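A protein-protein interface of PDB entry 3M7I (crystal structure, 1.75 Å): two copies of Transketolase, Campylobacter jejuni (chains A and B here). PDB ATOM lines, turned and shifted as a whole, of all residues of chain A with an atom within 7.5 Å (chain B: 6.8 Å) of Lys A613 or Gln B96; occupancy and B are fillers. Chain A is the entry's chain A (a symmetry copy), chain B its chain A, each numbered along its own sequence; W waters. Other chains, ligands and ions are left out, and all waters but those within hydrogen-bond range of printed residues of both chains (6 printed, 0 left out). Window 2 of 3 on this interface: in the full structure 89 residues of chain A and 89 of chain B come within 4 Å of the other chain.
No position is printed for both chains.
Of the 15 pairs that touch across the chains among the printed residues, none has its exchanged pair printed and touching as well.
Water W4 lies within hydrogen-bond range of O of Ala B27, NZ of Lys A613, OE2 of Glu A451 and NE2 of Gln B96.
Water W5 lies within hydrogen-bond range of the side-chain carboxylate (OD2) of Asp A616, the side-chain amide oxygen (OE1) of Gln B96, the backbone NH (N) of Lys A613 and the backbone NH (N) of Leu B97.
Water W1 bridges OG of Ser B29 and OE1 of Glu A451.
Water W6 lies within hydrogen-bond range of the backbone NH of His B98, the side-chain carboxylate of Glu A610 and the backbone carbonyl oxygen of Ser A611.
Water W3 lies within hydrogen-bond range of O of Gln B96, OG of Ser B99 and O of Ser A611.
Water W2 bridges the side-chain amino group (NZ) of Lys A613 and the backbone carbonyl oxygen (O) of Lys B26.
Among the printed residues, merely in contact across the chains: Glu A451 with Ser B29 (3.3 Å), Glu A451 with Arg B95 (3.4 Å), Glu A451 with Gly B103 (3.5 Å), Glu A610 with Leu B97 (3.7 Å), Ser A611 with Arg B95 (3.7 Å), Ser A611 with Pro B102 (3.5 Å), Gly A612 with Arg B95 (3.4 Å), Gly A612 with Leu B97 (3.7 Å), Lys A613 with Ala B27 (3.8 Å), Lys A613 with Gln B96 (3.4 Å) and Asp A616 with Leu B97 (3.8 Å).
The guanidinium group (NH1) of Arg B95 is in salt-bridge range of the side-chain carboxylate (OD1) of Asp A452, 2.9 Å away.
N of Leu B97 sits close to O of Ser A611.
The backbone NH (N) of Gly B103 is in hydrogen-bond range of the side-chain hydroxyl (OG) of Ser A611.
O of Ser A611 sits close to O of Gln B96 (3.4 Å).
Hydrophobic or aromatic side chains of chain B that line the printed part of chain A: Leu B97 and Pro B102.
Along chain B the printed residues that touch a printed residue of chain A span positions 27 to 103.
Among the printed residues, 15 pairs touch across the chains.
The side-chain hydroxyl of Ser B29 sits at hydrogen-bond distance from the guanidinium group of Arg B95.
The backbone NH (N) of Arg B95 is in hydrogen-bond range of the backbone carbonyl oxygen (O) of Thr B101.
The backbone carbonyl oxygen (O) of Gly B103 is in hydrogen-bond range of the guanidinium group (NH2) of Arg B95 (3.2 Å).
O of Gln B96 sits at hydrogen-bond distance from OG of Ser B99 (3.3 Å).
The side-chain hydroxyl of Ser A611 lies within hydrogen-bond range of the backbone carbonyl oxygen of Glu A451 (2.7 Å).
O of Glu A610 sits at hydrogen-bond distance from NE2 of Gln A457, 2.9 Å away.
Of chain B, only Ala B27 (3.8 Å) and Gln B96 (3.4 Å) come within 4 Å of Lys A613.
Of the printed residues of chain A, Gln B96 touches Ser A611 (3.4 Å) and Lys A613 (3.4 Å).
Of the printed residues of chain B, Glu A451 touches Ser B29, Arg B95 and Gly B103.
Of the printed residues of chain A, Ala B27 touches Lys A613.
Of the printed residues of chain A, Ser B29 touches Glu A451.
Of the printed residues of chain A, Leu B97 touches Glu A610, Ser A611, Gly A612 and Asp A616.
Of the printed residues of chain B, Glu A610 touches Leu B97 (3.7 Å).
Lys A615 touches none of the printed residues of chain B.
The nearest printed residue of chain A that does not touch Gly B103 is Asp A452 (4.3 Å).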
ATOM      1  N   ILE A 447      -7.373 -16.983  27.283  1.00  0.00           N
ATOM      2  CA  ILE A 447      -8.373 -17.918  26.714  1.00  0.00           C
ATOM      3  C   ILE A 447      -8.729 -17.580  25.251  1.00  0.00           C
ATOM      4  O   ILE A 447      -9.193 -18.466  24.521  1.00  0.00           O
ATOM      5  CB  ILE A 447      -9.638 -18.001  27.590  1.00  0.00           C
ATOM      6  CG1 ILE A 447     -10.235 -16.609  27.859  1.00  0.00           C
ATOM      7  CG2 ILE A 447      -9.346 -18.756  28.884  1.00  0.00           C
ATOM      8  CD1 ILE A 447     -11.667 -16.692  28.362  1.00  0.00           C
ATOM      9  N   GLY A 448      -8.478 -16.355  24.805  1.00  0.00           N
ATOM     10  CA  GLY A 448      -8.661 -15.974  23.378  1.00  0.00           C
ATOM     11  C   GLY A 448      -7.878 -16.840  22.420  1.00  0.00           C
ATOM     12  O   GLY A 448      -8.160 -16.913  21.205  1.00  0.00           O
ATOM     13  N   VAL A 449      -6.866 -17.487  22.952  1.00  0.00           N
ATOM     14  CA  VAL A 449      -6.153 -18.521  22.195  1.00  0.00           C
ATOM     15  C   VAL A 449      -7.079 -19.544  21.569  1.00  0.00           C
ATOM     16  O   VAL A 449      -6.857 -19.936  20.399  1.00  0.00           O
ATOM     17  CB  VAL A 449      -5.137 -19.204  23.067  1.00  0.00           C
ATOM     18  CG1 VAL A 449      -4.653 -20.474  22.388  1.00  0.00           C
ATOM     19  CG2 VAL A 449      -3.930 -18.220  23.366  1.00  0.00           C
ATOM     20  N   GLY A 450      -8.080 -20.005  22.334  1.00  0.00           N
ATOM     21  CA  GLY A 450      -9.129 -20.863  21.755  1.00  0.00           C
ATOM     22  C   GLY A 450      -8.811 -22.335  21.728  1.00  0.00           C
ATOM     23  O   GLY A 450      -8.638 -22.982  22.775  1.00  0.00           O
ATOM     24  N   GLU A 451      -8.690 -22.901  20.536  1.00  0.00           N
ATOM     25  CA  GLU A 451      -8.738 -24.325  20.409  1.00  0.00           C
ATOM     26  C   GLU A 451      -7.620 -25.117  21.059  1.00  0.00           C
ATOM     27  O   GLU A 451      -7.839 -26.241  21.462  1.00  0.00           O
ATOM     28  CB  GLU A 451      -8.768 -24.732  18.900  1.00  0.00           C
ATOM     29  CG  GLU A 451     -10.127 -24.387  18.244  1.00  0.00           C
ATOM     30  CD  GLU A 451     -10.185 -22.993  17.587  1.00  0.00           C
ATOM     31  OE1 GLU A 451      -9.438 -22.056  17.935  1.00  0.00           O
ATOM     32  OE2 GLU A 451     -10.999 -22.899  16.635  1.00  0.00           O
ATOM     33  N   ASP A 452      -6.448 -24.534  21.146  1.00  0.00           N
ATOM     34  CA  ASP A 452      -5.330 -25.242  21.769  1.00  0.00           C
ATOM     35  C   ASP A 452      -5.590 -25.622  23.235  1.00  0.00           C
ATOM     36  O   ASP A 452      -4.991 -26.570  23.777  1.00  0.00           O
ATOM     37  CB  ASP A 452      -4.046 -24.419  21.641  1.00  0.00           C
ATOM     38  CG  ASP A 452      -3.305 -24.602  20.308  1.00  0.00           C
ATOM     39  OD1 ASP A 452      -3.628 -25.492  19.501  1.00  0.00           O
ATOM     40  OD2 ASP A 452      -2.359 -23.819  20.094  1.00  0.00           O
ATOM     41  N   GLN A 457      -3.597 -21.702  27.627  1.00  0.00           N
ATOM     42  CA  GLN A 457      -4.309 -20.471  27.921  1.00  0.00           C
ATOM     43  C   GLN A 457      -3.851 -19.941  29.275  1.00  0.00           C
ATOM     44  O   GLN A 457      -4.137 -20.562  30.283  1.00  0.00           O
ATOM     45  CB  GLN A 457      -5.794 -20.767  27.927  1.00  0.00           C
ATOM     46  CG  GLN A 457      -6.374 -21.028  26.557  1.00  0.00           C
ATOM     47  CD  GLN A 457      -7.754 -21.677  26.587  1.00  0.00           C
ATOM     48  OE1 GLN A 457      -8.237 -22.082  27.624  1.00  0.00           O
ATOM     49  NE2 GLN A 457      -8.388 -21.812  25.423  1.00  0.00           N
ATOM     50  N   GLU A 610     -10.653 -23.618  28.451  1.00  0.00           N
ATOM     51  CA  GLU A 610     -11.321 -24.684  27.688  1.00  0.00           C
ATOM     52  C   GLU A 610     -10.868 -24.665  26.278  1.00  0.00           C
ATOM     53  O   GLU A 610     -10.692 -23.613  25.701  1.00  0.00           O
ATOM     54  CB  GLU A 610     -12.843 -24.453  27.674  1.00  0.00           C
ATOM     55  CG  GLU A 610     -13.540 -24.693  28.966  1.00  0.00           C
ATOM     56  CD  GLU A 610     -13.505 -26.121  29.476  1.00  0.00           C
ATOM     57  OE1 GLU A 610     -13.260 -27.107  28.719  1.00  0.00           O
ATOM     58  OE2 GLU A 610     -13.743 -26.243  30.696  1.00  0.00           O
ATOM     59  N   SER A 611     -10.843 -25.843  25.681  1.00  0.00           N
ATOM     60  CA  SER A 611     -10.571 -25.979  24.270  1.00  0.00           C
ATOM     61  C   SER A 611     -11.838 -25.705  23.488  1.00  0.00           C
ATOM     62  O   SER A 611     -12.816 -26.416  23.672  1.00  0.00           O
ATOM     63  CB  SER A 611     -10.098 -27.404  23.940  1.00  0.00           C
ATOM     64  OG  SER A 611      -9.913 -27.563  22.552  1.00  0.00           O
ATOM     65  N   GLY A 612     -11.778 -24.645  22.671  1.00  0.00           N
ATOM     66  CA  GLY A 612     -12.860 -24.257  21.781  1.00  0.00           C
ATOM     67  C   GLY A 612     -12.551 -23.044  20.929  1.00  0.00           C
ATOM     68  O   GLY A 612     -11.573 -22.307  21.125  1.00  0.00           O
ATOM     69  N   LYS A 613     -13.475 -22.743  19.999  1.00  0.00           N
ATOM     70  CA  LYS A 613     -13.377 -21.501  19.285  1.00  0.00           C
ATOM     71  C   LYS A 613     -13.306 -20.311  20.244  1.00  0.00           C
ATOM     72  O   LYS A 613     -14.091 -20.240  21.207  1.00  0.00           O
ATOM     73  CB  LYS A 613     -14.562 -21.357  18.304  1.00  0.00           C
ATOM     74  CG  LYS A 613     -14.502 -22.312  17.108  1.00  0.00           C
ATOM     75  CD  LYS A 613     -15.634 -22.004  16.083  1.00  0.00           C
ATOM     76  CE  LYS A 613     -15.971 -23.238  15.226  1.00  0.00           C
ATOM     77  NZ  LYS A 613     -14.835 -23.684  14.400  1.00  0.00           N
ATOM     78  N   ASP A 614     -12.418 -19.358  19.973  1.00  0.00           N
ATOM     79  CA  ASP A 614     -12.238 -18.131  20.841  1.00  0.00           C
ATOM     80  C   ASP A 614     -13.549 -17.483  21.223  1.00  0.00           C
ATOM     81  O   ASP A 614     -13.771 -17.224  22.413  1.00  0.00           O
ATOM     82  CB  ASP A 614     -11.295 -17.054  20.250  1.00  0.00           C
ATOM     83  CG  ASP A 614     -11.653 -16.604  18.832  1.00  0.00           C
ATOM     84  OD1 ASP A 614     -12.675 -17.037  18.216  1.00  0.00           O
ATOM     85  OD2 ASP A 614     -10.860 -15.794  18.312  1.00  0.00           O
ATOM     86  N   LYS A 615     -14.437 -17.293  20.268  1.00  0.00           N
ATOM     87  CA  LYS A 615     -15.754 -16.645  20.626  1.00  0.00           C
ATOM     88  C   LYS A 615     -16.588 -17.519  21.552  1.00  0.00           C
ATOM     89  O   LYS A 615     -17.192 -16.995  22.495  1.00  0.00           O
ATOM     90  CB  LYS A 615     -16.494 -16.250  19.362  1.00  0.00           C
ATOM     91  CG  LYS A 615     -15.903 -14.927  18.974  1.00  0.00           C
ATOM     92  CD  LYS A 615     -16.072 -14.449  17.522  1.00  0.00           C
ATOM     93  CE  LYS A 615     -15.181 -13.190  17.301  1.00  0.00           C
ATOM     94  NZ  LYS A 615     -15.764 -12.165  16.398  1.00  0.00           N
ATOM     95  N   ASP A 616     -16.534 -18.830  21.366  1.00  0.00           N
ATOM     96  CA  ASP A 616     -17.249 -19.779  22.260  1.00  0.00           C
ATOM     97  C   ASP A 616     -16.649 -19.745  23.681  1.00  0.00           C
ATOM     98  O   ASP A 616     -17.356 -19.782  24.693  1.00  0.00           O
ATOM     99  CB  ASP A 616     -17.169 -21.193  21.704  1.00  0.00           C
ATOM    100  CG  ASP A 616     -18.004 -21.398  20.462  1.00  0.00           C
ATOM    101  OD1 ASP A 616     -18.792 -20.458  20.152  1.00  0.00           O
ATOM    102  OD2 ASP A 616     -17.861 -22.493  19.825  1.00  0.00           O
ATOM    103  N   VAL A 617     -15.314 -19.719  23.774  1.00  0.00           N
ATOM    104  CA  VAL A 617     -14.683 -19.756  25.115  1.00  0.00           C
ATOM    105  C   VAL A 617     -14.894 -18.435  25.859  1.00  0.00           C
ATOM    106  O   VAL A 617     -15.181 -18.407  27.025  1.00  0.00           O
ATOM    107  CB  VAL A 617     -13.191 -20.054  24.980  1.00  0.00           C
ATOM    108  CG1 VAL A 617     -12.558 -20.135  26.350  1.00  0.00           C
ATOM    109  CG2 VAL A 617     -12.992 -21.318  24.232  1.00  0.00           C
ATOM    110  N   PHE A 618     -14.775 -17.314  25.167  1.00  0.00           N
ATOM    111  CA  PHE A 618     -14.977 -16.029  25.826  1.00  0.00           C
ATOM    112  C   PHE A 618     -16.416 -15.965  26.354  1.00  0.00           C
ATOM    113  O   PHE A 618     -16.644 -15.435  27.465  1.00  0.00           O
ATOM    114  CB  PHE A 618     -14.749 -14.815  24.854  1.00  0.00           C
ATOM    115  CG  PHE A 618     -13.364 -14.321  24.813  1.00  0.00           C
ATOM    116  CD1 PHE A 618     -12.719 -13.837  25.960  1.00  0.00           C
ATOM    117  CD2 PHE A 618     -12.646 -14.323  23.593  1.00  0.00           C
ATOM    118  CE1 PHE A 618     -11.412 -13.353  25.887  1.00  0.00           C
ATOM    119  CE2 PHE A 618     -11.322 -13.815  23.513  1.00  0.00           C
ATOM    120  CZ  PHE A 618     -10.702 -13.359  24.649  1.00  0.00           C
ATOM    121  N   GLU A 619     -17.365 -16.476  25.565  1.00  0.00           N
ATOM    122  CA  GLU A 619     -18.794 -16.431  25.988  1.00  0.00           C
ATOM    123  C   GLU A 619     -19.012 -17.336  27.230  1.00  0.00           C
ATOM    124  O   GLU A 619     -19.584 -16.948  28.249  1.00  0.00           O
ATOM    125  CB  GLU A 619     -19.706 -16.829  24.802  1.00  0.00           C
ATOM    126  CG  GLU A 619     -21.174 -16.861  25.204  1.00  0.00           C
ATOM    127  CD  GLU A 619     -21.701 -15.472  25.534  1.00  0.00           C
ATOM    128  OE1 GLU A 619     -21.287 -14.504  24.876  1.00  0.00           O
ATOM    129  OE2 GLU A 619     -22.554 -15.318  26.449  1.00  0.00           O
ATOM    130  N   LYS B  26     -12.246 -30.429   9.824  1.00  0.00           N
ATOM    131  CA  LYS B  26     -13.618 -30.073  10.230  1.00  0.00           C
ATOM    132  C   LYS B  26     -13.582 -28.984  11.292  1.00  0.00           C
ATOM    133  O   LYS B  26     -14.399 -28.081  11.308  1.00  0.00           O
ATOM    134  CB  LYS B  26     -14.353 -31.299  10.781  1.00  0.00           C
ATOM    135  CG  LYS B  26     -15.819 -31.054  11.131  1.00  0.00           C
ATOM    136  CD  LYS B  26     -16.602 -32.327  11.377  1.00  0.00           C
ATOM    137  CE  LYS B  26     -18.094 -32.002  11.525  1.00  0.00           C
ATOM    138  NZ  LYS B  26     -18.304 -31.376  12.861  1.00  0.00           N
ATOM    139  N   ALA B  27     -12.629 -29.116  12.225  1.00  0.00           N
ATOM    140  CA  ALA B  27     -12.354 -28.065  13.213  1.00  0.00           C
ATOM    141  C   ALA B  27     -11.773 -26.757  12.644  1.00  0.00           C
ATOM    142  O   ALA B  27     -11.805 -25.677  13.314  1.00  0.00           O
ATOM    143  CB  ALA B  27     -11.363 -28.637  14.349  1.00  0.00           C
ATOM    144  N   ASN B  28     -11.182 -26.826  11.438  1.00  0.00           N
ATOM    145  CA  ASN B  28     -10.402 -25.742  10.883  1.00  0.00           C
ATOM    146  C   ASN B  28      -9.317 -25.304  11.860  1.00  0.00           C
ATOM    147  O   ASN B  28      -8.987 -24.138  11.965  1.00  0.00           O
ATOM    148  CB  ASN B  28     -11.274 -24.550  10.459  1.00  0.00           C
ATOM    149  CG  ASN B  28     -10.602 -23.705   9.399  1.00  0.00           C
ATOM    150  OD1 ASN B  28      -9.748 -24.213   8.630  1.00  0.00           O
ATOM    151  ND2 ASN B  28     -10.943 -22.428   9.361  1.00  0.00           N
ATOM    152  N   SER B  29      -8.771 -26.296  12.566  1.00  0.00           N
ATOM    153  CA  SER B  29      -7.790 -26.008  13.589  1.00  0.00           C
ATOM    154  C   SER B  29      -7.100 -27.285  13.981  1.00  0.00           C
ATOM    155  O   SER B  29      -7.698 -28.343  14.081  1.00  0.00           O
ATOM    156  CB  SER B  29      -8.503 -25.418  14.819  1.00  0.00           C
ATOM    157  OG  SER B  29      -7.609 -25.135  15.866  1.00  0.00           O
ATOM    158  N   LYS B  92     -15.698 -35.981  15.503  1.00  0.00           N
ATOM    159  CA  LYS B  92     -16.203 -34.880  14.722  1.00  0.00           C
ATOM    160  C   LYS B  92     -16.364 -33.575  15.510  1.00  0.00           C
ATOM    161  O   LYS B  92     -16.592 -32.512  14.899  1.00  0.00           O
ATOM    162  CB  LYS B  92     -17.571 -35.244  14.082  1.00  0.00           C
ATOM    163  CG  LYS B  92     -17.499 -36.431  13.083  1.00  0.00           C
ATOM    164  CD  LYS B  92     -18.945 -36.919  12.624  1.00  0.00           C
ATOM    165  CE  LYS B  92     -18.769 -38.128  11.620  1.00  0.00           C
ATOM    166  NZ  LYS B  92     -20.047 -38.694  11.086  1.00  0.00           N
ATOM    167  N   ASN B  93     -16.252 -33.633  16.838  1.00  0.00           N
ATOM    168  CA  ASN B  93     -16.248 -32.396  17.629  1.00  0.00           C
ATOM    169  C   ASN B  93     -14.886 -32.040  18.211  1.00  0.00           C
ATOM    170  O   ASN B  93     -14.799 -31.304  19.187  1.00  0.00           O
ATOM    171  CB  ASN B  93     -17.271 -32.545  18.681  1.00  0.00           C
ATOM    172  CG  ASN B  93     -18.708 -32.405  18.079  1.00  0.00           C
ATOM    173  OD1 ASN B  93     -19.327 -33.375  17.702  1.00  0.00           O
ATOM    174  ND2 ASN B  93     -19.192 -31.194  18.026  1.00  0.00           N
ATOM    175  N   PHE B  94     -13.828 -32.557  17.544  1.00  0.00           N
ATOM    176  CA  PHE B  94     -12.449 -32.093  17.812  1.00  0.00           C
ATOM    177  C   PHE B  94     -12.332 -30.595  17.939  1.00  0.00           C
ATOM    178  O   PHE B  94     -12.778 -29.790  17.082  1.00  0.00           O
ATOM    179  CB  PHE B  94     -11.544 -32.532  16.670  1.00  0.00           C
ATOM    180  CG  PHE B  94     -10.063 -32.316  16.894  1.00  0.00           C
ATOM    181  CD1 PHE B  94      -9.414 -32.893  17.980  1.00  0.00           C
ATOM    182  CD2 PHE B  94      -9.304 -31.637  15.923  1.00  0.00           C
ATOM    183  CE1 PHE B  94      -7.991 -32.746  18.100  1.00  0.00           C
ATOM    184  CE2 PHE B  94      -7.906 -31.502  16.042  1.00  0.00           C
ATOM    185  CZ  PHE B  94      -7.268 -32.037  17.144  1.00  0.00           C
ATOM    186  N   ARG B  95     -11.767 -30.215  19.079  1.00  0.00           N
ATOM    187  CA  ARG B  95     -11.393 -28.896  19.389  1.00  0.00           C
ATOM    188  C   ARG B  95     -12.584 -27.949  19.681  1.00  0.00           C
ATOM    189  O   ARG B  95     -12.401 -26.770  19.587  1.00  0.00           O
ATOM    190  CB  ARG B  95     -10.476 -28.237  18.379  1.00  0.00           C
ATOM    191  CG  ARG B  95      -8.939 -28.739  18.540  1.00  0.00           C
ATOM    192  CD  ARG B  95      -7.961 -28.318  17.412  1.00  0.00           C
ATOM    193  NE  ARG B  95      -6.650 -28.647  17.920  1.00  0.00           N
ATOM    194  CZ  ARG B  95      -5.776 -27.754  18.347  1.00  0.00           C
ATOM    195  NH1 ARG B  95      -5.978 -26.476  18.139  1.00  0.00           N
ATOM    196  NH2 ARG B  95      -4.702 -28.188  19.008  1.00  0.00           N
ATOM    197  N   GLN B  96     -13.747 -28.534  19.845  1.00  0.00           N
ATOM    198  CA  GLN B  96     -14.940 -27.715  20.074  1.00  0.00           C
ATOM    199  C   GLN B  96     -15.242 -27.641  21.567  1.00  0.00           C
ATOM    200  O   GLN B  96     -15.056 -28.590  22.323  1.00  0.00           O
ATOM    201  CB  GLN B  96     -16.095 -28.315  19.320  1.00  0.00           C
ATOM    202  CG  GLN B  96     -15.842 -28.345  17.861  1.00  0.00           C
ATOM    203  CD  GLN B  96     -15.344 -27.006  17.293  1.00  0.00           C
ATOM    204  OE1 GLN B  96     -16.012 -25.929  17.351  1.00  0.00           O
ATOM    205  NE2 GLN B  96     -14.133 -27.051  16.750  1.00  0.00           N
ATOM    206  N   LEU B  97     -15.828 -26.520  21.957  1.00  0.00           N
ATOM    207  CA  LEU B  97     -16.162 -26.297  23.354  1.00  0.00           C
ATOM    208  C   LEU B  97     -16.951 -27.450  23.945  1.00  0.00           C
ATOM    209  O   LEU B  97     -17.974 -27.893  23.391  1.00  0.00           O
ATOM    210  CB  LEU B  97     -16.937 -24.986  23.455  1.00  0.00           C
ATOM    211  CG  LEU B  97     -17.250 -24.627  24.924  1.00  0.00           C
ATOM    212  CD1 LEU B  97     -15.967 -24.298  25.663  1.00  0.00           C
ATOM    213  CD2 LEU B  97     -18.218 -23.433  25.109  1.00  0.00           C
ATOM    214  N   HIS B  98     -16.454 -27.961  25.071  1.00  0.00           N
ATOM    215  CA  HIS B  98     -17.045 -29.027  25.838  1.00  0.00           C
ATOM    216  C   HIS B  98     -17.023 -30.424  25.213  1.00  0.00           C
ATOM    217  O   HIS B  98     -17.652 -31.346  25.749  1.00  0.00           O
ATOM    218  CB  HIS B  98     -18.471 -28.670  26.312  1.00  0.00           C
ATOM    219  CG  HIS B  98     -18.527 -27.410  27.140  1.00  0.00           C
ATOM    220  ND1 HIS B  98     -19.525 -26.473  26.984  1.00  0.00           N
ATOM    221  CD2 HIS B  98     -17.694 -26.915  28.096  1.00  0.00           C
ATOM    222  CE1 HIS B  98     -19.316 -25.467  27.818  1.00  0.00           C
ATOM    223  NE2 HIS B  98     -18.219 -25.705  28.510  1.00  0.00           N
ATOM    224  N   SER B  99     -16.245 -30.622  24.148  1.00  0.00           N
ATOM    225  CA  SER B  99     -16.107 -31.952  23.619  1.00  0.00           C
ATOM    226  C   SER B  99     -15.153 -32.799  24.472  1.00  0.00           C
ATOM    227  O   SER B  99     -14.408 -32.274  25.345  1.00  0.00           O
ATOM    228  CB  SER B  99     -15.594 -31.891  22.179  1.00  0.00           C
ATOM    229  OG  SER B  99     -14.181 -31.749  22.141  1.00  0.00           O
ATOM    230  N   LYS B 100     -15.149 -34.097  24.162  1.00  0.00           N
ATOM    231  CA  LYS B 100     -14.197 -35.098  24.727  1.00  0.00           C
ATOM    232  C   LYS B 100     -12.885 -35.182  23.955  1.00  0.00           C
ATOM    233  O   LYS B 100     -12.005 -35.979  24.344  1.00  0.00           O
ATOM    234  CB  LYS B 100     -14.871 -36.473  24.752  1.00  0.00           C
ATOM    235  CG  LYS B 100     -16.128 -36.574  25.642  1.00  0.00           C
ATOM    236  CD  LYS B 100     -16.809 -37.919  25.381  1.00  0.00           C
ATOM    237  CE  LYS B 100     -17.947 -38.233  26.354  1.00  0.00           C
ATOM    238  NZ  LYS B 100     -18.284 -39.739  26.310  1.00  0.00           N
ATOM    239  N   THR B 101     -12.747 -34.330  22.939  1.00  0.00           N
ATOM    240  CA  THR B 101     -11.566 -34.276  22.050  1.00  0.00           C
ATOM    241  C   THR B 101     -10.949 -32.877  21.986  1.00  0.00           C
ATOM    242  O   THR B 101     -10.890 -32.209  20.964  1.00  0.00           O
ATOM    243  CB  THR B 101     -12.000 -34.843  20.683  1.00  0.00           C
ATOM    244  OG1 THR B 101     -13.235 -34.170  20.334  1.00  0.00           O
ATOM    245  CG2 THR B 101     -12.232 -36.284  20.782  1.00  0.00           C
ATOM    246  N   PRO B 102     -10.466 -32.361  23.145  1.00  0.00           N
ATOM    247  CA  PRO B 102      -9.867 -31.068  23.155  1.00  0.00           C
ATOM    248  C   PRO B 102      -8.509 -31.011  22.423  1.00  0.00           C
ATOM    249  O   PRO B 102      -7.891 -32.070  22.142  1.00  0.00           O
ATOM    250  CB  PRO B 102      -9.625 -30.807  24.664  1.00  0.00           C
ATOM    251  CG  PRO B 102      -9.466 -32.160  25.246  1.00  0.00           C
ATOM    252  CD  PRO B 102     -10.451 -33.018  24.461  1.00  0.00           C
ATOM    253  N   GLY B 103      -8.084 -29.804  22.062  1.00  0.00           N
ATOM    254  CA  GLY B 103      -6.875 -29.560  21.212  1.00  0.00           C
ATOM    255  C   GLY B 103      -5.629 -30.273  21.674  1.00  0.00           C
ATOM    256  O   GLY B 103      -4.843 -30.797  20.856  1.00  0.00           O
HETATM  257  O   HOH W   1      -7.005 -22.541  16.318  1.00  0.00           O
HETATM  258  O   HOH W   2     -15.509 -26.023  13.100  1.00  0.00           O
HETATM  259  O   HOH W   3     -12.806 -29.659  23.494  1.00  0.00           O
HETATM  260  O   HOH W   4     -12.711 -24.756  15.545  1.00  0.00           O
HETATM  261  O   HOH W   5     -16.007 -24.314  19.833  1.00  0.00           O
HETATM  262  O   HOH W   6     -13.951 -27.569  26.021  1.00  0.00           O
